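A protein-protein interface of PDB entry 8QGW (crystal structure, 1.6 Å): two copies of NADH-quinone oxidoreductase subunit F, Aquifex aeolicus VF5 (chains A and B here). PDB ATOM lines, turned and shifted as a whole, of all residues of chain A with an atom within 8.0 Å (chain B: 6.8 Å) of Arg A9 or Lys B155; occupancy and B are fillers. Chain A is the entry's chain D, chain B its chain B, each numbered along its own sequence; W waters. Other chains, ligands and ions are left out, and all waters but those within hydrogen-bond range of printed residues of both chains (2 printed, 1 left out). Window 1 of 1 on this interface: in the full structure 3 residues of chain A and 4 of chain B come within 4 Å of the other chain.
The guanidinium group (NE) of Arg A9 is in hydrogen-bond range of the backbone carbonyl oxygen (O) of Lys B155 (3.0 Å).
The backbone carbonyl oxygen (O) of Ile A7 lies within hydrogen-bond range of the guanidinium group (NH2) of Arg A9, 3.1 Å away.
CB of Arg A9 touches O of Lys B154 (3.8 Å). CD2 of Leu B163 touches CZ of Arg A9, 3.6 Å away. Pro A26 touches Lys B154 (CG to O, 3.96 Å).
Of the printed residues of chain B, Arg A9 touches Lys B154 (3.8 Å), Lys B155 (3.0 Å) and Leu B163 (3.6 Å). Lys B155 touches just one residue of chain A: Arg A9 (3.0 Å). Of the printed residues of chain A, Leu B163 touches Arg A9 (3.6 Å). Printed residues of chain A within 4 Å of Lys B154: Arg A9 and Pro A26. Pro A5 touches none of the printed residues of chain B. The nearest printed residue of chain B that does not touch Arg A9 is Phe B157 (4.05 Å). The nearest residue of chain A that does not touch Lys B155 is Pro A26 (5.2 Å). The nearest printed residue of chain B that does not touch Pro A26 is Lys B153 (4.1 Å).
Of the 15 printed residues of chain A, 2 touch a printed residue of chain B. Hydrophobic or aromatic side chains of chain A that line the printed part of chain B: Pro A26. Printed residues of chain B that touch a printed residue of chain A: Lys B154, Lys B155 and Leu B163.
No position is printed for both chains.
Water W2 bridges O of Lys B154 (2.6 Å) and O of Ile A10 (2.9 Å). Water W1 lies within hydrogen-bond range of the backbone carbonyl oxygen of Arg A9 and the side-chain amino group of Lys B155.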
ATOM      1  N   PRO A   5      -2.982  24.915   1.317  1.00  0.00           N
ATOM      2  CA  PRO A   5      -2.398  24.939   2.655  1.00  0.00           C
ATOM      3  C   PRO A   5      -0.877  24.781   2.612  1.00  0.00           C
ATOM      4  O   PRO A   5      -0.328  24.205   1.666  1.00  0.00           O
ATOM      5  CB  PRO A   5      -3.035  23.729   3.364  1.00  0.00           C
ATOM      6  CG  PRO A   5      -4.307  23.453   2.590  1.00  0.00           C
ATOM      7  CD  PRO A   5      -3.950  23.803   1.155  1.00  0.00           C
ATOM      8  N   ALA A   6      -0.230  25.305   3.652  1.00  0.00           N
ATOM      9  CA  ALA A   6       1.218  25.229   3.774  1.00  0.00           C
ATOM     10  C   ALA A   6       1.671  23.771   3.871  1.00  0.00           C
ATOM     11  O   ALA A   6       1.065  22.975   4.577  1.00  0.00           O
ATOM     12  CB  ALA A   6       1.668  26.036   4.968  1.00  0.00           C
ATOM     13  N   ILE A   7       2.737  23.424   3.130  1.00  0.00           N
ATOM     14  CA  ILE A   7       3.355  22.102   3.155  1.00  0.00           C
ATOM     15  C   ILE A   7       4.839  22.323   3.417  1.00  0.00           C
ATOM     16  O   ILE A   7       5.442  23.125   2.720  1.00  0.00           O
ATOM     17  CB  ILE A   7       3.241  21.397   1.792  1.00  0.00           C
ATOM     18  CG1 ILE A   7       1.809  21.303   1.269  1.00  0.00           C
ATOM     19  CG2 ILE A   7       3.945  20.040   1.795  1.00  0.00           C
ATOM     20  CD1 ILE A   7       1.744  20.820  -0.169  1.00  0.00           C
ATOM     21  N   PRO A   8       5.496  21.605   4.354  1.00  0.00           N
ATOM     22  CA  PRO A   8       6.941  21.753   4.495  1.00  0.00           C
ATOM     23  C   PRO A   8       7.646  21.265   3.230  1.00  0.00           C
ATOM     24  O   PRO A   8       7.134  20.402   2.506  1.00  0.00           O
ATOM     25  CB  PRO A   8       7.309  20.930   5.735  1.00  0.00           C
ATOM     26  CG  PRO A   8       6.126  20.048   6.011  1.00  0.00           C
ATOM     27  CD  PRO A   8       4.933  20.586   5.248  1.00  0.00           C
ATOM     28  N   ARG A   9       8.808  21.882   2.936  1.00  0.00           N
ATOM     29  CA  ARG A   9       9.492  21.607   1.679  1.00  0.00           C
ATOM     30  C   ARG A   9      10.495  20.461   1.866  1.00  0.00           C
ATOM     31  O   ARG A   9      11.669  20.677   2.185  1.00  0.00           O
ATOM     32  CB  ARG A   9      10.156  22.880   1.142  1.00  0.00           C
ATOM     33  CG  ARG A   9       9.241  23.786   0.318  1.00  0.00           C
ATOM     34  CD  ARG A   9       8.185  24.491   1.146  1.00  0.00           C
ATOM     35  NE  ARG A   9       8.773  25.426   2.100  1.00  0.00           N
ATOM     36  CZ  ARG A   9       8.097  26.075   3.048  1.00  0.00           C
ATOM     37  NH1 ARG A   9       8.691  27.029   3.743  1.00  0.00           N
ATOM     38  NH2 ARG A   9       6.820  25.799   3.264  1.00  0.00           N
ATOM     39  N   ILE A  10      10.006  19.236   1.677  1.00  0.00           N
ATOM     40  CA  ILE A  10      10.800  18.028   1.841  1.00  0.00           C
ATOM     41  C   ILE A  10      11.844  18.010   0.723  1.00  0.00           C
ATOM     42  O   ILE A  10      11.513  18.261  -0.438  1.00  0.00           O
ATOM     43  CB  ILE A  10       9.866  16.799   1.814  1.00  0.00           C
ATOM     44  CG1 ILE A  10       8.909  16.833   3.013  1.00  0.00           C
ATOM     45  CG2 ILE A  10      10.647  15.493   1.742  1.00  0.00           C
ATOM     46  CD1 ILE A  10       7.775  15.838   2.936  1.00  0.00           C
ATOM     47  N   TYR A  11      13.088  17.692   1.092  1.00  0.00           N
ATOM     48  CA  TYR A  11      14.166  17.589   0.121  1.00  0.00           C
ATOM     49  C   TYR A  11      13.964  16.330  -0.719  1.00  0.00           C
ATOM     50  O   TYR A  11      13.596  15.294  -0.199  1.00  0.00           O
ATOM     51  CB  TYR A  11      15.527  17.493   0.804  1.00  0.00           C
ATOM     52  CG  TYR A  11      16.665  17.308  -0.172  1.00  0.00           C
ATOM     53  CD1 TYR A  11      16.934  18.283  -1.120  1.00  0.00           C
ATOM     54  CD2 TYR A  11      17.485  16.194  -0.130  1.00  0.00           C
ATOM     55  CE1 TYR A  11      17.965  18.130  -2.035  1.00  0.00           C
ATOM     56  CE2 TYR A  11      18.528  16.028  -1.025  1.00  0.00           C
ATOM     57  CZ  TYR A  11      18.792  17.019  -1.959  1.00  0.00           C
ATOM     58  OH  TYR A  11      19.819  16.880  -2.873  1.00  0.00           O
ATOM     59  N   ALA A  12      14.275  16.424  -2.016  1.00  0.00           N
ATOM     60  CA  ALA A  12      14.084  15.307  -2.931  1.00  0.00           C
ATOM     61  C   ALA A  12      15.231  15.301  -3.951  1.00  0.00           C
ATOM     62  O   ALA A  12      15.613  16.352  -4.475  1.00  0.00           O
ATOM     63  CB  ALA A  12      12.737  15.417  -3.588  1.00  0.00           C
ATOM     64  N   LYS A  25      11.485  19.349  -7.476  1.00  0.00           N
ATOM     65  CA  LYS A  25      11.282  20.757  -7.176  1.00  0.00           C
ATOM     66  C   LYS A  25      10.023  20.893  -6.323  1.00  0.00           C
ATOM     67  O   LYS A  25       8.969  20.373  -6.706  1.00  0.00           O
ATOM     68  CB  LYS A  25      11.148  21.573  -8.467  1.00  0.00           C
ATOM     69  CG  LYS A  25      12.429  22.115  -9.082  1.00  0.00           C
ATOM     70  CD  LYS A  25      13.656  21.237  -9.026  1.00  0.00           C
ATOM     71  CE  LYS A  25      14.907  21.978  -9.451  1.00  0.00           C
ATOM     72  NZ  LYS A  25      14.679  22.767 -10.689  1.00  0.00           N
ATOM     73  N   PRO A  26      10.097  21.548  -5.139  1.00  0.00           N
ATOM     74  CA  PRO A  26       9.011  21.518  -4.161  1.00  0.00           C
ATOM     75  C   PRO A  26       7.896  22.525  -4.421  1.00  0.00           C
ATOM     76  O   PRO A  26       7.719  23.492  -3.680  1.00  0.00           O
ATOM     77  CB  PRO A  26       9.756  21.821  -2.853  1.00  0.00           C
ATOM     78  CG  PRO A  26      10.807  22.819  -3.296  1.00  0.00           C
ATOM     79  CD  PRO A  26      11.285  22.263  -4.626  1.00  0.00           C
ATOM     80  N   ARG A  27       7.124  22.242  -5.476  1.00  0.00           N
ATOM     81  CA  ARG A  27       5.969  23.046  -5.833  1.00  0.00           C
ATOM     82  C   ARG A  27       5.021  22.228  -6.711  1.00  0.00           C
ATOM     83  O   ARG A  27       5.406  21.194  -7.254  1.00  0.00           O
ATOM     84  CB  ARG A  27       6.395  24.306  -6.583  1.00  0.00           C
ATOM     85  CG  ARG A  27       7.153  24.048  -7.878  1.00  0.00           C
ATOM     86  CD  ARG A  27       7.534  25.337  -8.611  1.00  0.00           C
ATOM     87  NE  ARG A  27       8.267  25.060  -9.834  1.00  0.00           N
ATOM     88  CZ  ARG A  27       7.695  24.691 -10.991  1.00  0.00           C
ATOM     89  NH1 ARG A  27       8.412  24.524 -12.097  1.00  0.00           N
ATOM     90  NH2 ARG A  27       6.391  24.502 -11.031  1.00  0.00           N
ATOM     91  N   ILE A 105       4.973  13.319  -2.080  1.00  0.00           N
ATOM     92  CA  ILE A 105       5.705  14.258  -2.912  1.00  0.00           C
ATOM     93  C   ILE A 105       5.273  14.098  -4.378  1.00  0.00           C
ATOM     94  O   ILE A 105       5.262  15.090  -5.105  1.00  0.00           O
ATOM     95  CB  ILE A 105       7.229  14.277  -2.715  1.00  0.00           C
ATOM     96  CG1 ILE A 105       7.889  13.031  -3.271  1.00  0.00           C
ATOM     97  CG2 ILE A 105       7.686  14.590  -1.277  1.00  0.00           C
ATOM     98  CD1 ILE A 105       9.365  13.238  -3.510  1.00  0.00           C
ATOM     99  N   ARG A 109       3.329  17.471  -5.846  1.00  0.00           N
ATOM    100  CA  ARG A 109       4.192  18.214  -6.762  1.00  0.00           C
ATOM    101  C   ARG A 109       3.978  17.830  -8.221  1.00  0.00           C
ATOM    102  O   ARG A 109       4.165  18.675  -9.086  1.00  0.00           O
ATOM    103  CB  ARG A 109       5.663  17.998  -6.428  1.00  0.00           C
ATOM    104  CG  ARG A 109       6.018  18.371  -5.005  1.00  0.00           C
ATOM    105  CD  ARG A 109       7.430  17.973  -4.628  1.00  0.00           C
ATOM    106  NE  ARG A 109       7.651  18.360  -3.240  1.00  0.00           N
ATOM    107  CZ  ARG A 109       8.834  18.341  -2.632  1.00  0.00           C
ATOM    108  NH1 ARG A 109       8.942  18.764  -1.375  1.00  0.00           N
ATOM    109  NH2 ARG A 109       9.893  17.928  -3.307  1.00  0.00           N
ATOM    110  N   PRO A 261      17.971  14.543   5.324  1.00  0.00           N
ATOM    111  CA  PRO A 261      16.718  13.795   5.312  1.00  0.00           C
ATOM    112  C   PRO A 261      15.857  14.257   4.132  1.00  0.00           C
ATOM    113  O   PRO A 261      15.864  15.450   3.791  1.00  0.00           O
ATOM    114  CB  PRO A 261      16.113  14.136   6.681  1.00  0.00           C
ATOM    115  CG  PRO A 261      16.646  15.509   6.962  1.00  0.00           C
ATOM    116  CD  PRO A 261      18.069  15.475   6.452  1.00  0.00           C
ATOM    117  N   GLY A 262      15.171  13.307   3.490  1.00  0.00           N
ATOM    118  CA  GLY A 262      14.340  13.595   2.334  1.00  0.00           C
ATOM    119  C   GLY A 262      14.040  12.337   1.526  1.00  0.00           C
ATOM    120  O   GLY A 262      14.269  11.231   2.023  1.00  0.00           O
ATOM    121  N   ILE B  31      21.498  27.258   6.611  1.00  0.00           N
ATOM    122  CA  ILE B  31      20.098  27.674   6.601  1.00  0.00           C
ATOM    123  C   ILE B  31      19.362  27.228   7.865  1.00  0.00           C
ATOM    124  O   ILE B  31      18.449  27.917   8.306  1.00  0.00           O
ATOM    125  CB  ILE B  31      19.363  27.224   5.317  1.00  0.00           C
ATOM    126  CG1 ILE B  31      18.109  28.076   5.082  1.00  0.00           C
ATOM    127  CG2 ILE B  31      19.033  25.737   5.374  1.00  0.00           C
ATOM    128  CD1 ILE B  31      17.539  28.017   3.689  1.00  0.00           C
ATOM    129  N   ASP B  32      19.707  26.072   8.438  1.00  0.00           N
ATOM    130  CA  ASP B  32      19.022  25.599   9.634  1.00  0.00           C
ATOM    131  C   ASP B  32      19.267  26.567  10.789  1.00  0.00           C
ATOM    132  O   ASP B  32      18.327  26.904  11.502  1.00  0.00           O
ATOM    133  CB  ASP B  32      19.402  24.153   9.982  1.00  0.00           C
ATOM    134  CG  ASP B  32      18.767  23.077   9.096  1.00  0.00           C
ATOM    135  OD1 ASP B  32      17.937  23.396   8.208  1.00  0.00           O
ATOM    136  OD2 ASP B  32      19.077  21.903   9.335  1.00  0.00           O
ATOM    137  N   LEU B  35      17.183  29.667  10.056  1.00  0.00           N
ATOM    138  CA  LEU B  35      15.762  29.425  10.316  1.00  0.00           C
ATOM    139  C   LEU B  35      15.463  29.401  11.818  1.00  0.00           C
ATOM    140  O   LEU B  35      14.412  29.860  12.251  1.00  0.00           O
ATOM    141  CB  LEU B  35      15.354  28.097   9.662  1.00  0.00           C
ATOM    142  CG  LEU B  35      15.317  28.113   8.134  1.00  0.00           C
ATOM    143  CD1 LEU B  35      15.213  26.714   7.579  1.00  0.00           C
ATOM    144  CD2 LEU B  35      14.159  28.937   7.605  1.00  0.00           C
ATOM    145  N   TYR B  40      13.865  34.037   7.170  1.00  0.00           N
ATOM    146  CA  TYR B  40      12.942  33.830   6.057  1.00  0.00           C
ATOM    147  C   TYR B  40      11.494  34.063   6.460  1.00  0.00           C
ATOM    148  O   TYR B  40      10.630  34.065   5.584  1.00  0.00           O
ATOM    149  CB  TYR B  40      13.167  32.478   5.372  1.00  0.00           C
ATOM    150  CG  TYR B  40      14.407  32.449   4.511  1.00  0.00           C
ATOM    151  CD1 TYR B  40      14.481  33.169   3.323  1.00  0.00           C
ATOM    152  CD2 TYR B  40      15.516  31.700   4.869  1.00  0.00           C
ATOM    153  CE1 TYR B  40      15.611  33.143   2.523  1.00  0.00           C
ATOM    154  CE2 TYR B  40      16.664  31.671   4.089  1.00  0.00           C
ATOM    155  CZ  TYR B  40      16.721  32.397   2.913  1.00  0.00           C
ATOM    156  OH  TYR B  40      17.875  32.370   2.140  1.00  0.00           O
ATOM    157  N   GLU B  44       8.369  35.608   4.180  1.00  0.00           N
ATOM    158  CA  GLU B  44       7.006  35.098   4.138  1.00  0.00           C
ATOM    159  C   GLU B  44       5.998  36.236   4.337  1.00  0.00           C
ATOM    160  O   GLU B  44       4.979  36.273   3.661  1.00  0.00           O
ATOM    161  CB  GLU B  44       6.798  34.030   5.207  1.00  0.00           C
ATOM    162  CG  GLU B  44       7.668  32.806   5.031  1.00  0.00           C
ATOM    163  CD  GLU B  44       7.417  31.801   6.139  1.00  0.00           C
ATOM    164  OE1 GLU B  44       6.395  31.083   6.066  1.00  0.00           O
ATOM    165  OE2 GLU B  44       8.177  31.809   7.120  1.00  0.00           O
ATOM    166  N   GLU B 150      21.611  27.249  -3.145  1.00  0.00           N
ATOM    167  CA  GLU B 150      21.068  25.905  -3.270  1.00  0.00           C
ATOM    168  C   GLU B 150      20.224  25.510  -2.051  1.00  0.00           C
ATOM    169  O   GLU B 150      19.185  24.879  -2.224  1.00  0.00           O
ATOM    170  CB  GLU B 150      22.187  24.887  -3.522  1.00  0.00           C
ATOM    171  CG  GLU B 150      22.834  25.019  -4.898  1.00  0.00           C
ATOM    172  CD  GLU B 150      21.861  25.124  -6.072  1.00  0.00           C
ATOM    173  OE1 GLU B 150      20.939  24.287  -6.138  1.00  0.00           O
ATOM    174  OE2 GLU B 150      22.012  26.075  -6.902  1.00  0.00           O
ATOM    175  N   GLU B 151      20.661  25.853  -0.823  1.00  0.00           N
ATOM    176  CA  GLU B 151      19.851  25.616   0.372  1.00  0.00           C
ATOM    177  C   GLU B 151      18.503  26.346   0.281  1.00  0.00           C
ATOM    178  O   GLU B 151      17.464  25.795   0.659  1.00  0.00           O
ATOM    179  CB  GLU B 151      20.541  26.101   1.658  1.00  0.00           C
ATOM    180  CG  GLU B 151      21.802  25.348   2.058  1.00  0.00           C
ATOM    181  CD  GLU B 151      22.451  25.919   3.326  1.00  0.00           C
ATOM    182  OE1 GLU B 151      22.405  25.218   4.372  1.00  0.00           O
ATOM    183  OE2 GLU B 151      22.982  27.060   3.310  1.00  0.00           O
ATOM    184  N   ALA B 152      18.522  27.602  -0.161  1.00  0.00           N
ATOM    185  CA  ALA B 152      17.309  28.397  -0.285  1.00  0.00           C
ATOM    186  C   ALA B 152      16.363  27.739  -1.292  1.00  0.00           C
ATOM    187  O   ALA B 152      15.166  27.687  -1.058  1.00  0.00           O
ATOM    188  CB  ALA B 152      17.617  29.828  -0.671  1.00  0.00           C
ATOM    189  N   LYS B 153      16.919  27.183  -2.375  1.00  0.00           N
ATOM    190  CA  LYS B 153      16.120  26.461  -3.358  1.00  0.00           C
ATOM    191  C   LYS B 153      15.493  25.204  -2.752  1.00  0.00           C
ATOM    192  O   LYS B 153      14.299  24.954  -2.965  1.00  0.00           O
ATOM    193  CB  LYS B 153      16.973  26.156  -4.594  1.00  0.00           C
ATOM    194  CG  LYS B 153      17.456  27.392  -5.343  1.00  0.00           C
ATOM    195  CD  LYS B 153      18.043  27.119  -6.718  1.00  0.00           C
ATOM    196  CE  LYS B 153      17.011  26.610  -7.705  1.00  0.00           C
ATOM    197  NZ  LYS B 153      17.536  26.578  -9.091  1.00  0.00           N
ATOM    198  N   LYS B 154      16.289  24.421  -2.000  1.00  0.00           N
ATOM    199  CA  LYS B 154      15.798  23.231  -1.312  1.00  0.00           C
ATOM    200  C   LYS B 154      14.559  23.573  -0.493  1.00  0.00           C
ATOM    201  O   LYS B 154      13.590  22.816  -0.478  1.00  0.00           O
ATOM    202  CB  LYS B 154      16.828  22.620  -0.348  1.00  0.00           C
ATOM    203  CG  LYS B 154      16.222  21.899   0.859  1.00  0.00           C
ATOM    204  CD  LYS B 154      17.214  21.402   1.910  1.00  0.00           C
ATOM    205  CE  LYS B 154      18.226  22.464   2.315  1.00  0.00           C
ATOM    206  NZ  LYS B 154      18.934  22.072   3.559  1.00  0.00           N
ATOM    207  N   LYS B 155      14.617  24.711   0.202  1.00  0.00           N
ATOM    208  CA  LYS B 155      13.596  25.092   1.161  1.00  0.00           C
ATOM    209  C   LYS B 155      12.454  25.874   0.525  1.00  0.00           C
ATOM    210  O   LYS B 155      11.563  26.289   1.253  1.00  0.00           O
ATOM    211  CB  LYS B 155      14.228  25.902   2.299  1.00  0.00           C
ATOM    212  CG  LYS B 155      15.086  25.077   3.240  1.00  0.00           C
ATOM    213  CD  LYS B 155      14.287  24.073   4.007  1.00  0.00           C
ATOM    214  CE  LYS B 155      15.018  23.579   5.237  1.00  0.00           C
ATOM    215  NZ  LYS B 155      14.277  22.475   5.884  1.00  0.00           N
ATOM    216  N   GLY B 156      12.475  26.081  -0.801  1.00  0.00           N
ATOM    217  CA  GLY B 156      11.367  26.724  -1.488  1.00  0.00           C
ATOM    218  C   GLY B 156      11.335  28.250  -1.403  1.00  0.00           C
ATOM    219  O   GLY B 156      10.292  28.849  -1.660  1.00  0.00           O
ATOM    220  N   PHE B 157      12.472  28.891  -1.096  1.00  0.00           N
ATOM    221  CA  PHE B 157      12.524  30.347  -1.050  1.00  0.00           C
ATOM    222  C   PHE B 157      12.961  30.957  -2.387  1.00  0.00           C
ATOM    223  O   PHE B 157      12.914  32.180  -2.526  1.00  0.00           O
ATOM    224  CB  PHE B 157      13.452  30.779   0.090  1.00  0.00           C
ATOM    225  CG  PHE B 157      13.030  30.268   1.441  1.00  0.00           C
ATOM    226  CD1 PHE B 157      11.743  30.483   1.914  1.00  0.00           C
ATOM    227  CD2 PHE B 157      13.929  29.597   2.263  1.00  0.00           C
ATOM    228  CE1 PHE B 157      11.351  30.023   3.164  1.00  0.00           C
ATOM    229  CE2 PHE B 157      13.527  29.126   3.507  1.00  0.00           C
ATOM    230  CZ  PHE B 157      12.237  29.328   3.948  1.00  0.00           C
ATOM    231  N   LEU B 158      13.427  30.114  -3.324  1.00  0.00           N
ATOM    232  CA  LEU B 158      13.799  30.495  -4.681  1.00  0.00           C
ATOM    233  C   LEU B 158      13.166  29.519  -5.669  1.00  0.00           C
ATOM    234  O   LEU B 158      12.715  28.429  -5.293  1.00  0.00           O
ATOM    235  CB  LEU B 158      15.325  30.486  -4.818  1.00  0.00           C
ATOM    236  CG  LEU B 158      16.058  31.643  -4.136  1.00  0.00           C
ATOM    237  CD1 LEU B 158      17.566  31.454  -4.174  1.00  0.00           C
ATOM    238  CD2 LEU B 158      15.710  32.967  -4.788  1.00  0.00           C
ATOM    239  N   LEU B 163       6.597  29.856  -2.472  1.00  0.00           N
ATOM    240  CA  LEU B 163       5.635  29.694  -1.386  1.00  0.00           C
ATOM    241  C   LEU B 163       4.218  30.046  -1.845  1.00  0.00           C
ATOM    242  O   LEU B 163       3.417  30.613  -1.096  1.00  0.00           O
ATOM    243  CB  LEU B 163       6.078  30.562  -0.208  1.00  0.00           C
ATOM    244  CG  LEU B 163       7.495  30.300   0.316  1.00  0.00           C
ATOM    245  CD1 LEU B 163       7.871  31.296   1.409  1.00  0.00           C
ATOM    246  CD2 LEU B 163       7.640  28.873   0.830  1.00  0.00           C
HETATM  247  O   HOH W   1      14.140  20.545   3.555  1.00  0.00           O
HETATM  248  O   HOH W   2      12.782  20.599  -1.590  1.00  0.00           O
